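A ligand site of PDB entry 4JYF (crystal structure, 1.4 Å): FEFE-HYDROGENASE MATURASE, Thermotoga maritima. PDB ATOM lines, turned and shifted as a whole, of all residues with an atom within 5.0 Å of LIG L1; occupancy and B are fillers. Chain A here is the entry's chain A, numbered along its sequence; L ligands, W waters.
O of Ile 231 sits at hydrogen-bond distance from N4 of LIG L1 (2.8 Å). The guanidinium group (NH2) of Arg 180 is in salt-bridge range of an oxygen (O2) of LIG L1, at 3.0 Å. O of Leu 305 lies within hydrogen-bond range of N4 of LIG L1, at 3.5 Å. The backbone carbonyl oxygen (O) of Tyr 69 sits at hydrogen-bond distance from a nitrogen (N4) of LIG L1 (2.9 Å). N1 of LIG L1 sits close to O of Ser 108 (3.2 Å). NH1 of Arg 159 is in hydrogen-bond range of O5 of LIG L1 (3.1 Å). SG of Cys 70 is bound to FE4 of LG2 L2 (2.2 Å). A nitrogen (N5) of LIG L1 is in hydrogen-bond range of the backbone NH (N) of Ile 231 (3.0 Å). OE2 of Glu 161 is in hydrogen-bond range of O4 of LIG L1, at 2.5 Å.
The backbone NH (N) of Ser 108 is in hydrogen-bond range of the backbone carbonyl oxygen (O) of Ser 136 (3.3 Å). NE2 of Gln 107 sits at hydrogen-bond distance from OG of Ser 136 (3.0 Å). NE of Arg 180 is in hydrogen-bond range of O of Arg 159 (2.7 Å). N of Met 199 sits at hydrogen-bond distance from O of Glu 161 (3.2 Å). NE of Arg 172 is in hydrogen-bond range of OH of Tyr 69. The side-chain carboxylate (OE2) of Glu 161 lies within salt-bridge range of the guanidinium group (NH2) of Arg 180 (3.2 Å). N of Ala 270 sits at hydrogen-bond distance from OH of Tyr 306 (3.1 Å). OG of Ser 136 lies within hydrogen-bond range of O of Leu 157, 3.5 Å away.
A nitrogen (N1) of LIG L1 is bound to an iron atom (FE2) of LG2 L2, at 2.2 Å.
The side-chain sulfur (SD) of Met 199 lies close to a nitrogen (N6) of LIG L1. Merely in contact with LIG L1: Cys 70 (3.9 Å), Gln 107 (3.7 Å), Ser 136 (3.7 Å), Gly 138 (3.8 Å), Pro 229 (3.1 Å), Phe 230 (3.9 Å), Tyr 303 (3.4 Å) and Tyr 306 (3.7 Å). Hydrophobic or aromatic side chains that line LIG L1: Tyr 69, Met 199, Ile 231, Leu 305 and Tyr 306. Within 4 Å of LIG L1: Tyr 69, Cys 70, Gln 107, Ser 108, Ser 136, Gly 138, Arg 159, Glu 161, Arg 180, Met 199, Pro 229, Phe 230, Ile 231, Tyr 303, Leu 305 and Tyr 306. The nearest printed residue that does not touch LIG L1 is Leu 158 (4.04 Å).
Water W3 lies within hydrogen-bond range of an oxygen (O4) of LIG L1 and the backbone NH (N) of Arg 159. Water W2 lies within hydrogen-bond range of the backbone carbonyl oxygen (O) of Leu 157 (2.7 Å), an oxygen (O2) of LIG L1 (2.8 Å), the backbone NH (N) of Gly 138 (3.0 Å), the side-chain hydroxyl (OG) of Ser 136 (3.1 Å) and the backbone NH (N) of Leu 137 (3.3 Å). Water W1 lies within hydrogen-bond range of N6 of LIG L1 (2.8 Å), NH1 of Arg 159 (3.2 Å) and O of Pro 229 (3.4 Å). Water W5 lies within hydrogen-bond range of the side-chain carboxylate of Glu 110 (2.7 Å), the guanidinium group of Arg 180 (2.8 Å), the guanidinium group of Arg 172 (3.2 Å) and a sulfur (S4) of LG2 L2 (3.3 Å). Water W6 lies within hydrogen-bond range of the side-chain carboxylate (OE2) of Glu 161 (2.7 Å), the side-chain hydroxyl (OH) of Tyr 69 (2.8 Å), the guanidinium group (NE) of Arg 172 (3.1 Å) and a sulfur (S3) of LG2 L2 (3.3 Å).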
ATOM      1  N   TYR A  69     -24.981 -24.354 -21.554  1.00  0.00           N
ATOM      2  CA  TYR A  69     -25.030 -25.301 -22.689  1.00  0.00           C
ATOM      3  C   TYR A  69     -24.981 -26.765 -22.264  1.00  0.00           C
ATOM      4  O   TYR A  69     -25.303 -27.658 -23.054  1.00  0.00           O
ATOM      5  CB  TYR A  69     -23.867 -25.028 -23.648  1.00  0.00           C
ATOM      6  CG  TYR A  69     -22.543 -24.830 -22.991  1.00  0.00           C
ATOM      7  CD1 TYR A  69     -21.792 -25.917 -22.552  1.00  0.00           C
ATOM      8  CD2 TYR A  69     -22.021 -23.543 -22.789  1.00  0.00           C
ATOM      9  CE1 TYR A  69     -20.576 -25.725 -21.943  1.00  0.00           C
ATOM     10  CE2 TYR A  69     -20.818 -23.348 -22.179  1.00  0.00           C
ATOM     11  CZ  TYR A  69     -20.076 -24.433 -21.761  1.00  0.00           C
ATOM     12  OH  TYR A  69     -18.878 -24.174 -21.146  1.00  0.00           O
ATOM     13  N   CYS A  70     -24.559 -27.006 -21.033  1.00  0.00           N
ATOM     14  CA  CYS A  70     -24.142 -28.350 -20.628  1.00  0.00           C
ATOM     15  C   CYS A  70     -25.150 -29.152 -19.852  1.00  0.00           C
ATOM     16  O   CYS A  70     -25.667 -28.687 -18.828  1.00  0.00           O
ATOM     17  CB  CYS A  70     -22.887 -28.234 -19.776  1.00  0.00           C
ATOM     18  SG  CYS A  70     -22.122 -29.821 -19.327  1.00  0.00           S
ATOM     19  N   GLN A 107     -11.790 -37.507 -17.470  1.00  0.00           N
ATOM     20  CA  GLN A 107     -12.647 -36.341 -17.606  1.00  0.00           C
ATOM     21  C   GLN A 107     -13.815 -36.466 -16.625  1.00  0.00           C
ATOM     22  O   GLN A 107     -14.329 -37.557 -16.369  1.00  0.00           O
ATOM     23  CB  GLN A 107     -13.166 -36.171 -19.032  1.00  0.00           C
ATOM     24  CG  GLN A 107     -13.914 -34.843 -19.270  1.00  0.00           C
ATOM     25  CD  GLN A 107     -14.345 -34.652 -20.667  1.00  0.00           C
ATOM     26  OE1 GLN A 107     -15.360 -35.182 -21.061  1.00  0.00           O
ATOM     27  NE2 GLN A 107     -13.604 -33.862 -21.422  1.00  0.00           N
ATOM     28  N   SER A 108     -14.255 -35.312 -16.125  1.00  0.00           N
ATOM     29  CA  SER A 108     -15.409 -35.259 -15.225  1.00  0.00           C
ATOM     30  C   SER A 108     -16.078 -33.897 -15.272  1.00  0.00           C
ATOM     31  O   SER A 108     -15.512 -32.919 -15.761  1.00  0.00           O
ATOM     32  CB  SER A 108     -14.990 -35.588 -13.784  1.00  0.00           C
ATOM     33  OG  SER A 108     -14.028 -34.666 -13.306  1.00  0.00           O
ATOM     34  N   GLY A 109     -17.273 -33.845 -14.674  1.00  0.00           N
ATOM     35  CA  GLY A 109     -17.794 -32.577 -14.181  1.00  0.00           C
ATOM     36  C   GLY A 109     -16.824 -32.032 -13.145  1.00  0.00           C
ATOM     37  O   GLY A 109     -15.896 -32.729 -12.696  1.00  0.00           O
ATOM     38  N   GLU A 110     -16.995 -30.771 -12.783  1.00  0.00           N
ATOM     39  CA  GLU A 110     -16.230 -30.210 -11.683  1.00  0.00           C
ATOM     40  C   GLU A 110     -16.797 -30.748 -10.371  1.00  0.00           C
ATOM     41  O   GLU A 110     -17.587 -30.100  -9.684  1.00  0.00           O
ATOM     42  CB  GLU A 110     -16.245 -28.677 -11.738  1.00  0.00           C
ATOM     43  CG  GLU A 110     -15.414 -28.093 -12.880  1.00  0.00           C
ATOM     44  CD  GLU A 110     -15.090 -26.602 -12.717  1.00  0.00           C
ATOM     45  OE1 GLU A 110     -15.395 -26.043 -11.636  1.00  0.00           O
ATOM     46  OE2 GLU A 110     -14.526 -25.997 -13.663  1.00  0.00           O
ATOM     47  N   SER A 136      -8.930 -33.688 -17.663  1.00  0.00           N
ATOM     48  CA  SER A 136      -9.888 -32.729 -18.186  1.00  0.00           C
ATOM     49  C   SER A 136     -10.963 -32.581 -17.112  1.00  0.00           C
ATOM     50  O   SER A 136     -12.034 -33.156 -17.166  1.00  0.00           O
ATOM     51  CB  SER A 136     -10.475 -33.228 -19.502  1.00  0.00           C
ATOM     52  OG  SER A 136     -11.414 -32.328 -20.059  1.00  0.00           O
ATOM     53  N   LEU A 137     -10.620 -31.801 -16.084  1.00  0.00           N
ATOM     54  CA  LEU A 137     -11.417 -31.724 -14.835  1.00  0.00           C
ATOM     55  C   LEU A 137     -11.994 -30.335 -14.585  1.00  0.00           C
ATOM     56  O   LEU A 137     -12.633 -30.116 -13.540  1.00  0.00           O
ATOM     57  CB  LEU A 137     -10.569 -32.151 -13.635  1.00  0.00           C
ATOM     58  CG  LEU A 137      -9.767 -33.436 -13.765  1.00  0.00           C
ATOM     59  CD1 LEU A 137      -8.927 -33.742 -12.499  1.00  0.00           C
ATOM     60  CD2 LEU A 137     -10.661 -34.649 -14.155  1.00  0.00           C
ATOM     61  N   GLY A 138     -11.753 -29.405 -15.509  1.00  0.00           N
ATOM     62  CA  GLY A 138     -12.237 -28.027 -15.365  1.00  0.00           C
ATOM     63  C   GLY A 138     -11.237 -27.137 -14.618  1.00  0.00           C
ATOM     64  O   GLY A 138     -10.011 -27.382 -14.598  1.00  0.00           O
ATOM     65  N   LEU A 157      -6.626 -30.856 -20.732  1.00  0.00           N
ATOM     66  CA  LEU A 157      -7.577 -30.271 -21.678  1.00  0.00           C
ATOM     67  C   LEU A 157      -8.490 -29.298 -20.934  1.00  0.00           C
ATOM     68  O   LEU A 157      -9.171 -29.685 -19.976  1.00  0.00           O
ATOM     69  CB  LEU A 157      -8.435 -31.345 -22.319  1.00  0.00           C
ATOM     70  CG  LEU A 157      -7.707 -32.559 -22.895  1.00  0.00           C
ATOM     71  CD1 LEU A 157      -8.719 -33.537 -23.465  1.00  0.00           C
ATOM     72  CD2 LEU A 157      -6.673 -32.145 -23.937  1.00  0.00           C
ATOM     73  N   LEU A 158      -8.500 -28.064 -21.407  1.00  0.00           N
ATOM     74  CA  LEU A 158      -9.351 -27.037 -20.842  1.00  0.00           C
ATOM     75  C   LEU A 158      -9.797 -26.130 -21.976  1.00  0.00           C
ATOM     76  O   LEU A 158      -9.178 -25.087 -22.238  1.00  0.00           O
ATOM     77  CB  LEU A 158      -8.629 -26.278 -19.741  1.00  0.00           C
ATOM     78  CG  LEU A 158      -9.519 -25.416 -18.866  1.00  0.00           C
ATOM     79  CD1 LEU A 158     -10.386 -26.253 -17.921  1.00  0.00           C
ATOM     80  CD2 LEU A 158      -8.677 -24.388 -18.065  1.00  0.00           C
ATOM     81  N   ARG A 159     -10.846 -26.550 -22.700  1.00  0.00           N
ATOM     82  CA  ARG A 159     -11.295 -25.767 -23.841  1.00  0.00           C
ATOM     83  C   ARG A 159     -11.569 -24.329 -23.403  1.00  0.00           C
ATOM     84  O   ARG A 159     -12.153 -24.124 -22.348  1.00  0.00           O
ATOM     85  CB  ARG A 159     -12.535 -26.347 -24.465  1.00  0.00           C
ATOM     86  CG  ARG A 159     -12.269 -27.646 -25.165  1.00  0.00           C
ATOM     87  CD  ARG A 159     -13.535 -28.074 -25.787  1.00  0.00           C
ATOM     88  NE  ARG A 159     -13.411 -29.365 -26.448  1.00  0.00           N
ATOM     89  CZ  ARG A 159     -14.374 -29.861 -27.211  1.00  0.00           C
ATOM     90  NH1 ARG A 159     -15.500 -29.184 -27.352  1.00  0.00           N
ATOM     91  NH2 ARG A 159     -14.210 -31.043 -27.802  1.00  0.00           N
ATOM     92  N   GLU A 161     -13.653 -22.472 -24.896  1.00  0.00           N
ATOM     93  CA  GLU A 161     -15.112 -22.441 -25.157  1.00  0.00           C
ATOM     94  C   GLU A 161     -15.516 -21.358 -26.133  1.00  0.00           C
ATOM     95  O   GLU A 161     -16.126 -21.654 -27.152  1.00  0.00           O
ATOM     96  CB  GLU A 161     -15.951 -22.362 -23.878  1.00  0.00           C
ATOM     97  CG  GLU A 161     -15.508 -23.323 -22.797  1.00  0.00           C
ATOM     98  CD  GLU A 161     -15.643 -24.803 -23.139  1.00  0.00           C
ATOM     99  OE1 GLU A 161     -16.002 -25.173 -24.286  1.00  0.00           O
ATOM    100  OE2 GLU A 161     -15.389 -25.612 -22.208  1.00  0.00           O
ATOM    101  N   ARG A 172     -21.227 -19.094 -18.997  1.00  0.00           N
ATOM    102  CA  ARG A 172     -20.498 -19.747 -17.925  1.00  0.00           C
ATOM    103  C   ARG A 172     -20.532 -18.826 -16.720  1.00  0.00           C
ATOM    104  O   ARG A 172     -19.520 -18.214 -16.351  1.00  0.00           O
ATOM    105  CB  ARG A 172     -19.087 -20.095 -18.390  1.00  0.00           C
ATOM    106  CG  ARG A 172     -19.079 -20.833 -19.723  1.00  0.00           C
ATOM    107  CD  ARG A 172     -17.725 -21.358 -20.118  1.00  0.00           C
ATOM    108  NE  ARG A 172     -17.389 -22.437 -19.187  1.00  0.00           N
ATOM    109  CZ  ARG A 172     -16.424 -22.429 -18.294  1.00  0.00           C
ATOM    110  NH1 ARG A 172     -15.562 -21.428 -18.246  1.00  0.00           N
ATOM    111  NH2 ARG A 172     -16.331 -23.448 -17.412  1.00  0.00           N
ATOM    112  N   ARG A 180     -10.509 -18.472 -17.303  1.00  0.00           N
ATOM    113  CA  ARG A 180     -10.230 -19.621 -18.181  1.00  0.00           C
ATOM    114  C   ARG A 180      -8.834 -19.490 -18.811  1.00  0.00           C
ATOM    115  O   ARG A 180      -8.027 -20.433 -18.781  1.00  0.00           O
ATOM    116  CB  ARG A 180     -11.312 -19.725 -19.253  1.00  0.00           C
ATOM    117  CG  ARG A 180     -11.429 -21.058 -19.943  1.00  0.00           C
ATOM    118  CD  ARG A 180     -12.045 -22.099 -19.050  1.00  0.00           C
ATOM    119  NE  ARG A 180     -12.367 -23.318 -19.760  1.00  0.00           N
ATOM    120  CZ  ARG A 180     -12.934 -24.374 -19.195  1.00  0.00           C
ATOM    121  NH1 ARG A 180     -13.224 -24.384 -17.895  1.00  0.00           N
ATOM    122  NH2 ARG A 180     -13.182 -25.447 -19.911  1.00  0.00           N
ATOM    123  N   MET A 199     -16.473 -24.298 -28.931  1.00  0.00           N
ATOM    124  CA  MET A 199     -17.666 -24.770 -29.613  1.00  0.00           C
ATOM    125  C   MET A 199     -18.000 -23.808 -30.723  1.00  0.00           C
ATOM    126  O   MET A 199     -17.660 -22.619 -30.673  1.00  0.00           O
ATOM    127  CB  MET A 199     -18.847 -24.914 -28.666  1.00  0.00           C
ATOM    128  CG  MET A 199     -18.690 -26.076 -27.660  1.00  0.00           C
ATOM    129  SD  MET A 199     -19.968 -26.079 -26.379  1.00  0.00           S
ATOM    130  CE  MET A 199     -19.332 -24.813 -25.312  1.00  0.00           C
ATOM    131  N   PRO A 229     -19.193 -28.810 -32.654  1.00  0.00           N
ATOM    132  CA  PRO A 229     -20.399 -27.983 -32.719  1.00  0.00           C
ATOM    133  C   PRO A 229     -21.091 -27.947 -31.370  1.00  0.00           C
ATOM    134  O   PRO A 229     -21.018 -28.898 -30.617  1.00  0.00           O
ATOM    135  CB  PRO A 229     -21.259 -28.730 -33.710  1.00  0.00           C
ATOM    136  CG  PRO A 229     -20.866 -30.204 -33.488  1.00  0.00           C
ATOM    137  CD  PRO A 229     -19.377 -30.149 -33.226  1.00  0.00           C
ATOM    138  N   PHE A 230     -21.756 -26.843 -31.084  1.00  0.00           N
ATOM    139  CA  PHE A 230     -22.715 -26.787 -30.007  1.00  0.00           C
ATOM    140  C   PHE A 230     -23.926 -27.686 -30.340  1.00  0.00           C
ATOM    141  O   PHE A 230     -24.493 -27.605 -31.445  1.00  0.00           O
ATOM    142  CB  PHE A 230     -23.197 -25.354 -29.823  1.00  0.00           C
ATOM    143  CG  PHE A 230     -24.435 -25.243 -28.984  1.00  0.00           C
ATOM    144  CD1 PHE A 230     -24.424 -25.597 -27.639  1.00  0.00           C
ATOM    145  CD2 PHE A 230     -25.617 -24.788 -29.550  1.00  0.00           C
ATOM    146  CE1 PHE A 230     -25.559 -25.519 -26.891  1.00  0.00           C
ATOM    147  CE2 PHE A 230     -26.760 -24.694 -28.759  1.00  0.00           C
ATOM    148  CZ  PHE A 230     -26.713 -25.071 -27.445  1.00  0.00           C
ATOM    149  N   ILE A 231     -24.312 -28.534 -29.388  1.00  0.00           N
ATOM    150  CA  ILE A 231     -25.467 -29.404 -29.535  1.00  0.00           C
ATOM    151  C   ILE A 231     -26.432 -29.143 -28.361  1.00  0.00           C
ATOM    152  O   ILE A 231     -26.088 -29.411 -27.202  1.00  0.00           O
ATOM    153  CB  ILE A 231     -25.042 -30.894 -29.563  1.00  0.00           C
ATOM    154  CG1 ILE A 231     -24.115 -31.156 -30.755  1.00  0.00           C
ATOM    155  CG2 ILE A 231     -26.254 -31.827 -29.645  1.00  0.00           C
ATOM    156  CD1 ILE A 231     -23.449 -32.511 -30.765  1.00  0.00           C
ATOM    157  N   PRO A 232     -27.628 -28.583 -28.648  1.00  0.00           N
ATOM    158  CA  PRO A 232     -28.532 -28.240 -27.554  1.00  0.00           C
ATOM    159  C   PRO A 232     -29.006 -29.439 -26.762  1.00  0.00           C
ATOM    160  O   PRO A 232     -29.313 -30.495 -27.318  1.00  0.00           O
ATOM    161  CB  PRO A 232     -29.710 -27.591 -28.294  1.00  0.00           C
ATOM    162  CG  PRO A 232     -29.704 -28.225 -29.632  1.00  0.00           C
ATOM    163  CD  PRO A 232     -28.242 -28.328 -29.964  1.00  0.00           C
ATOM    164  N   ALA A 270     -18.636 -34.971 -30.696  1.00  0.00           N
ATOM    165  CA  ALA A 270     -19.731 -34.105 -31.133  1.00  0.00           C
ATOM    166  C   ALA A 270     -19.817 -34.053 -32.641  1.00  0.00           C
ATOM    167  O   ALA A 270     -20.921 -34.001 -33.186  1.00  0.00           O
ATOM    168  CB  ALA A 270     -19.581 -32.713 -30.511  1.00  0.00           C
ATOM    169  N   TYR A 303     -23.387 -39.656 -18.795  1.00  0.00           N
ATOM    170  CA  TYR A 303     -22.462 -38.537 -19.048  1.00  0.00           C
ATOM    171  C   TYR A 303     -22.921 -37.843 -20.319  1.00  0.00           C
ATOM    172  O   TYR A 303     -22.399 -38.086 -21.404  1.00  0.00           O
ATOM    173  CB  TYR A 303     -21.041 -39.017 -19.144  1.00  0.00           C
ATOM    174  CG  TYR A 303     -20.024 -37.908 -19.049  1.00  0.00           C
ATOM    175  CD1 TYR A 303     -19.587 -37.459 -17.805  1.00  0.00           C
ATOM    176  CD2 TYR A 303     -19.497 -37.316 -20.183  1.00  0.00           C
ATOM    177  CE1 TYR A 303     -18.643 -36.464 -17.698  1.00  0.00           C
ATOM    178  CE2 TYR A 303     -18.551 -36.335 -20.097  1.00  0.00           C
ATOM    179  CZ  TYR A 303     -18.125 -35.902 -18.845  1.00  0.00           C
ATOM    180  OH  TYR A 303     -17.169 -34.913 -18.753  1.00  0.00           O
ATOM    181  N   LEU A 305     -23.272 -34.510 -21.796  1.00  0.00           N
ATOM    182  CA  LEU A 305     -22.994 -33.083 -21.988  1.00  0.00           C
ATOM    183  C   LEU A 305     -24.013 -32.546 -22.989  1.00  0.00           C
ATOM    184  O   LEU A 305     -24.527 -31.449 -22.843  1.00  0.00           O
ATOM    185  CB  LEU A 305     -21.572 -32.900 -22.515  1.00  0.00           C
ATOM    186  CG  LEU A 305     -20.404 -33.446 -21.680  1.00  0.00           C
ATOM    187  CD1 LEU A 305     -19.110 -33.367 -22.541  1.00  0.00           C
ATOM    188  CD2 LEU A 305     -20.273 -32.726 -20.370  1.00  0.00           C
ATOM    189  N   TYR A 306     -24.254 -33.354 -24.031  1.00  0.00           N
ATOM    190  CA  TYR A 306     -25.255 -33.133 -25.046  1.00  0.00           C
ATOM    191  C   TYR A 306     -25.929 -34.479 -25.333  1.00  0.00           C
ATOM    192  O   TYR A 306     -25.354 -35.539 -25.010  1.00  0.00           O
ATOM    193  CB  TYR A 306     -24.617 -32.560 -26.323  1.00  0.00           C
ATOM    194  CG  TYR A 306     -23.402 -33.313 -26.795  1.00  0.00           C
ATOM    195  CD1 TYR A 306     -23.542 -34.460 -27.586  1.00  0.00           C
ATOM    196  CD2 TYR A 306     -22.133 -32.923 -26.426  1.00  0.00           C
ATOM    197  CE1 TYR A 306     -22.449 -35.158 -28.016  1.00  0.00           C
ATOM    198  CE2 TYR A 306     -21.019 -33.626 -26.851  1.00  0.00           C
ATOM    199  CZ  TYR A 306     -21.186 -34.767 -27.640  1.00  0.00           C
ATOM    200  OH  TYR A 306     -20.101 -35.494 -28.068  1.00  0.00           O
HETATM  201  N1  LIG L   1     -16.037 -29.954 -16.794  1.00  0.00           N
HETATM  202  C1  LIG L   1     -14.815 -29.928 -17.646  1.00  0.00           C
HETATM  203  C2  LIG L   1     -14.799 -31.147 -18.580  1.00  0.00           C
HETATM  204  C3  LIG L   1     -16.091 -31.667 -19.132  1.00  0.00           C
HETATM  205  S1  LIG L   1     -16.896 -30.564 -20.277  1.00  0.00           S
HETATM  206  C4  LIG L   1     -14.759 -28.606 -18.384  1.00  0.00           C
HETATM  207  O1  LIG L   1     -15.787 -27.893 -18.386  1.00  0.00           O
HETATM  208  O2  LIG L   1     -13.740 -28.241 -18.997  1.00  0.00           O
HETATM  209  C5  LIG L   1     -16.012 -31.077 -21.809  1.00  0.00           C
HETATM  210  C6  LIG L   1     -16.318 -30.203 -23.044  1.00  0.00           C
HETATM  211  O3  LIG L   1     -17.554 -30.577 -23.657  1.00  0.00           O
HETATM  212  C7  LIG L   1     -16.473 -28.708 -22.816  1.00  0.00           C
HETATM  213  O4  LIG L   1     -15.236 -28.032 -22.772  1.00  0.00           O
HETATM  214  C8  LIG L   1     -17.389 -28.227 -23.943  1.00  0.00           C
HETATM  215  O5  LIG L   1     -16.724 -27.595 -25.026  1.00  0.00           O
HETATM  216  C9  LIG L   1     -18.099 -29.525 -24.421  1.00  0.00           C
HETATM  217  N2  LIG L   1     -19.571 -29.435 -24.309  1.00  0.00           N
HETATM  218  C10 LIG L   1     -20.294 -29.249 -23.164  1.00  0.00           C
HETATM  219  N3  LIG L   1     -21.599 -29.158 -23.461  1.00  0.00           N
HETATM  220  C11 LIG L   1     -21.719 -29.211 -24.820  1.00  0.00           C
HETATM  221  C12 LIG L   1     -22.799 -29.187 -25.684  1.00  0.00           C
HETATM  222  N4  LIG L   1     -24.052 -28.978 -25.275  1.00  0.00           N
HETATM  223  N5  LIG L   1     -22.578 -29.309 -27.044  1.00  0.00           N
HETATM  224  C13 LIG L   1     -21.332 -29.493 -27.561  1.00  0.00           C
HETATM  225  N6  LIG L   1     -20.269 -29.554 -26.700  1.00  0.00           N
HETATM  226  C14 LIG L   1     -20.443 -29.415 -25.359  1.00  0.00           C
HETATM  227 FE1  LG2 L   2     -19.548 -26.556 -17.256  1.00  0.00          FE
HETATM  228 FE2  LG2 L   2     -17.722 -28.729 -17.539  1.00  0.00          FE
HETATM  229 FE3  LG2 L   2     -19.702 -28.607 -15.466  1.00  0.00          FE
HETATM  230 FE4  LG2 L   2     -20.515 -29.017 -17.990  1.00  0.00          FE
HETATM  231  S1  LG2 L   2     -19.215 -30.413 -16.824  1.00  0.00           S
HETATM  232  S2  LG2 L   2     -21.454 -27.586 -16.423  1.00  0.00           S
HETATM  233  S3  LG2 L   2     -18.999 -27.745 -19.183  1.00  0.00           S
HETATM  234  S4  LG2 L   2     -17.920 -27.137 -15.808  1.00  0.00           S
HETATM  235  O   HOH W   1     -18.283 -29.777 -28.712  1.00  0.00           O
HETATM  236  O   HOH W   2     -11.425 -29.688 -18.487  1.00  0.00           O
HETATM  237  O   HOH W   3     -12.819 -28.520 -21.636  1.00  0.00           O
HETATM  238  O   HOH W   4     -16.540 -32.992 -25.251  1.00  0.00           O
HETATM  239  O   HOH W   5     -14.815 -26.003 -16.317  1.00  0.00           O
HETATM  240  O   HOH W   6     -16.767 -25.411 -19.865  1.00  0.00           O
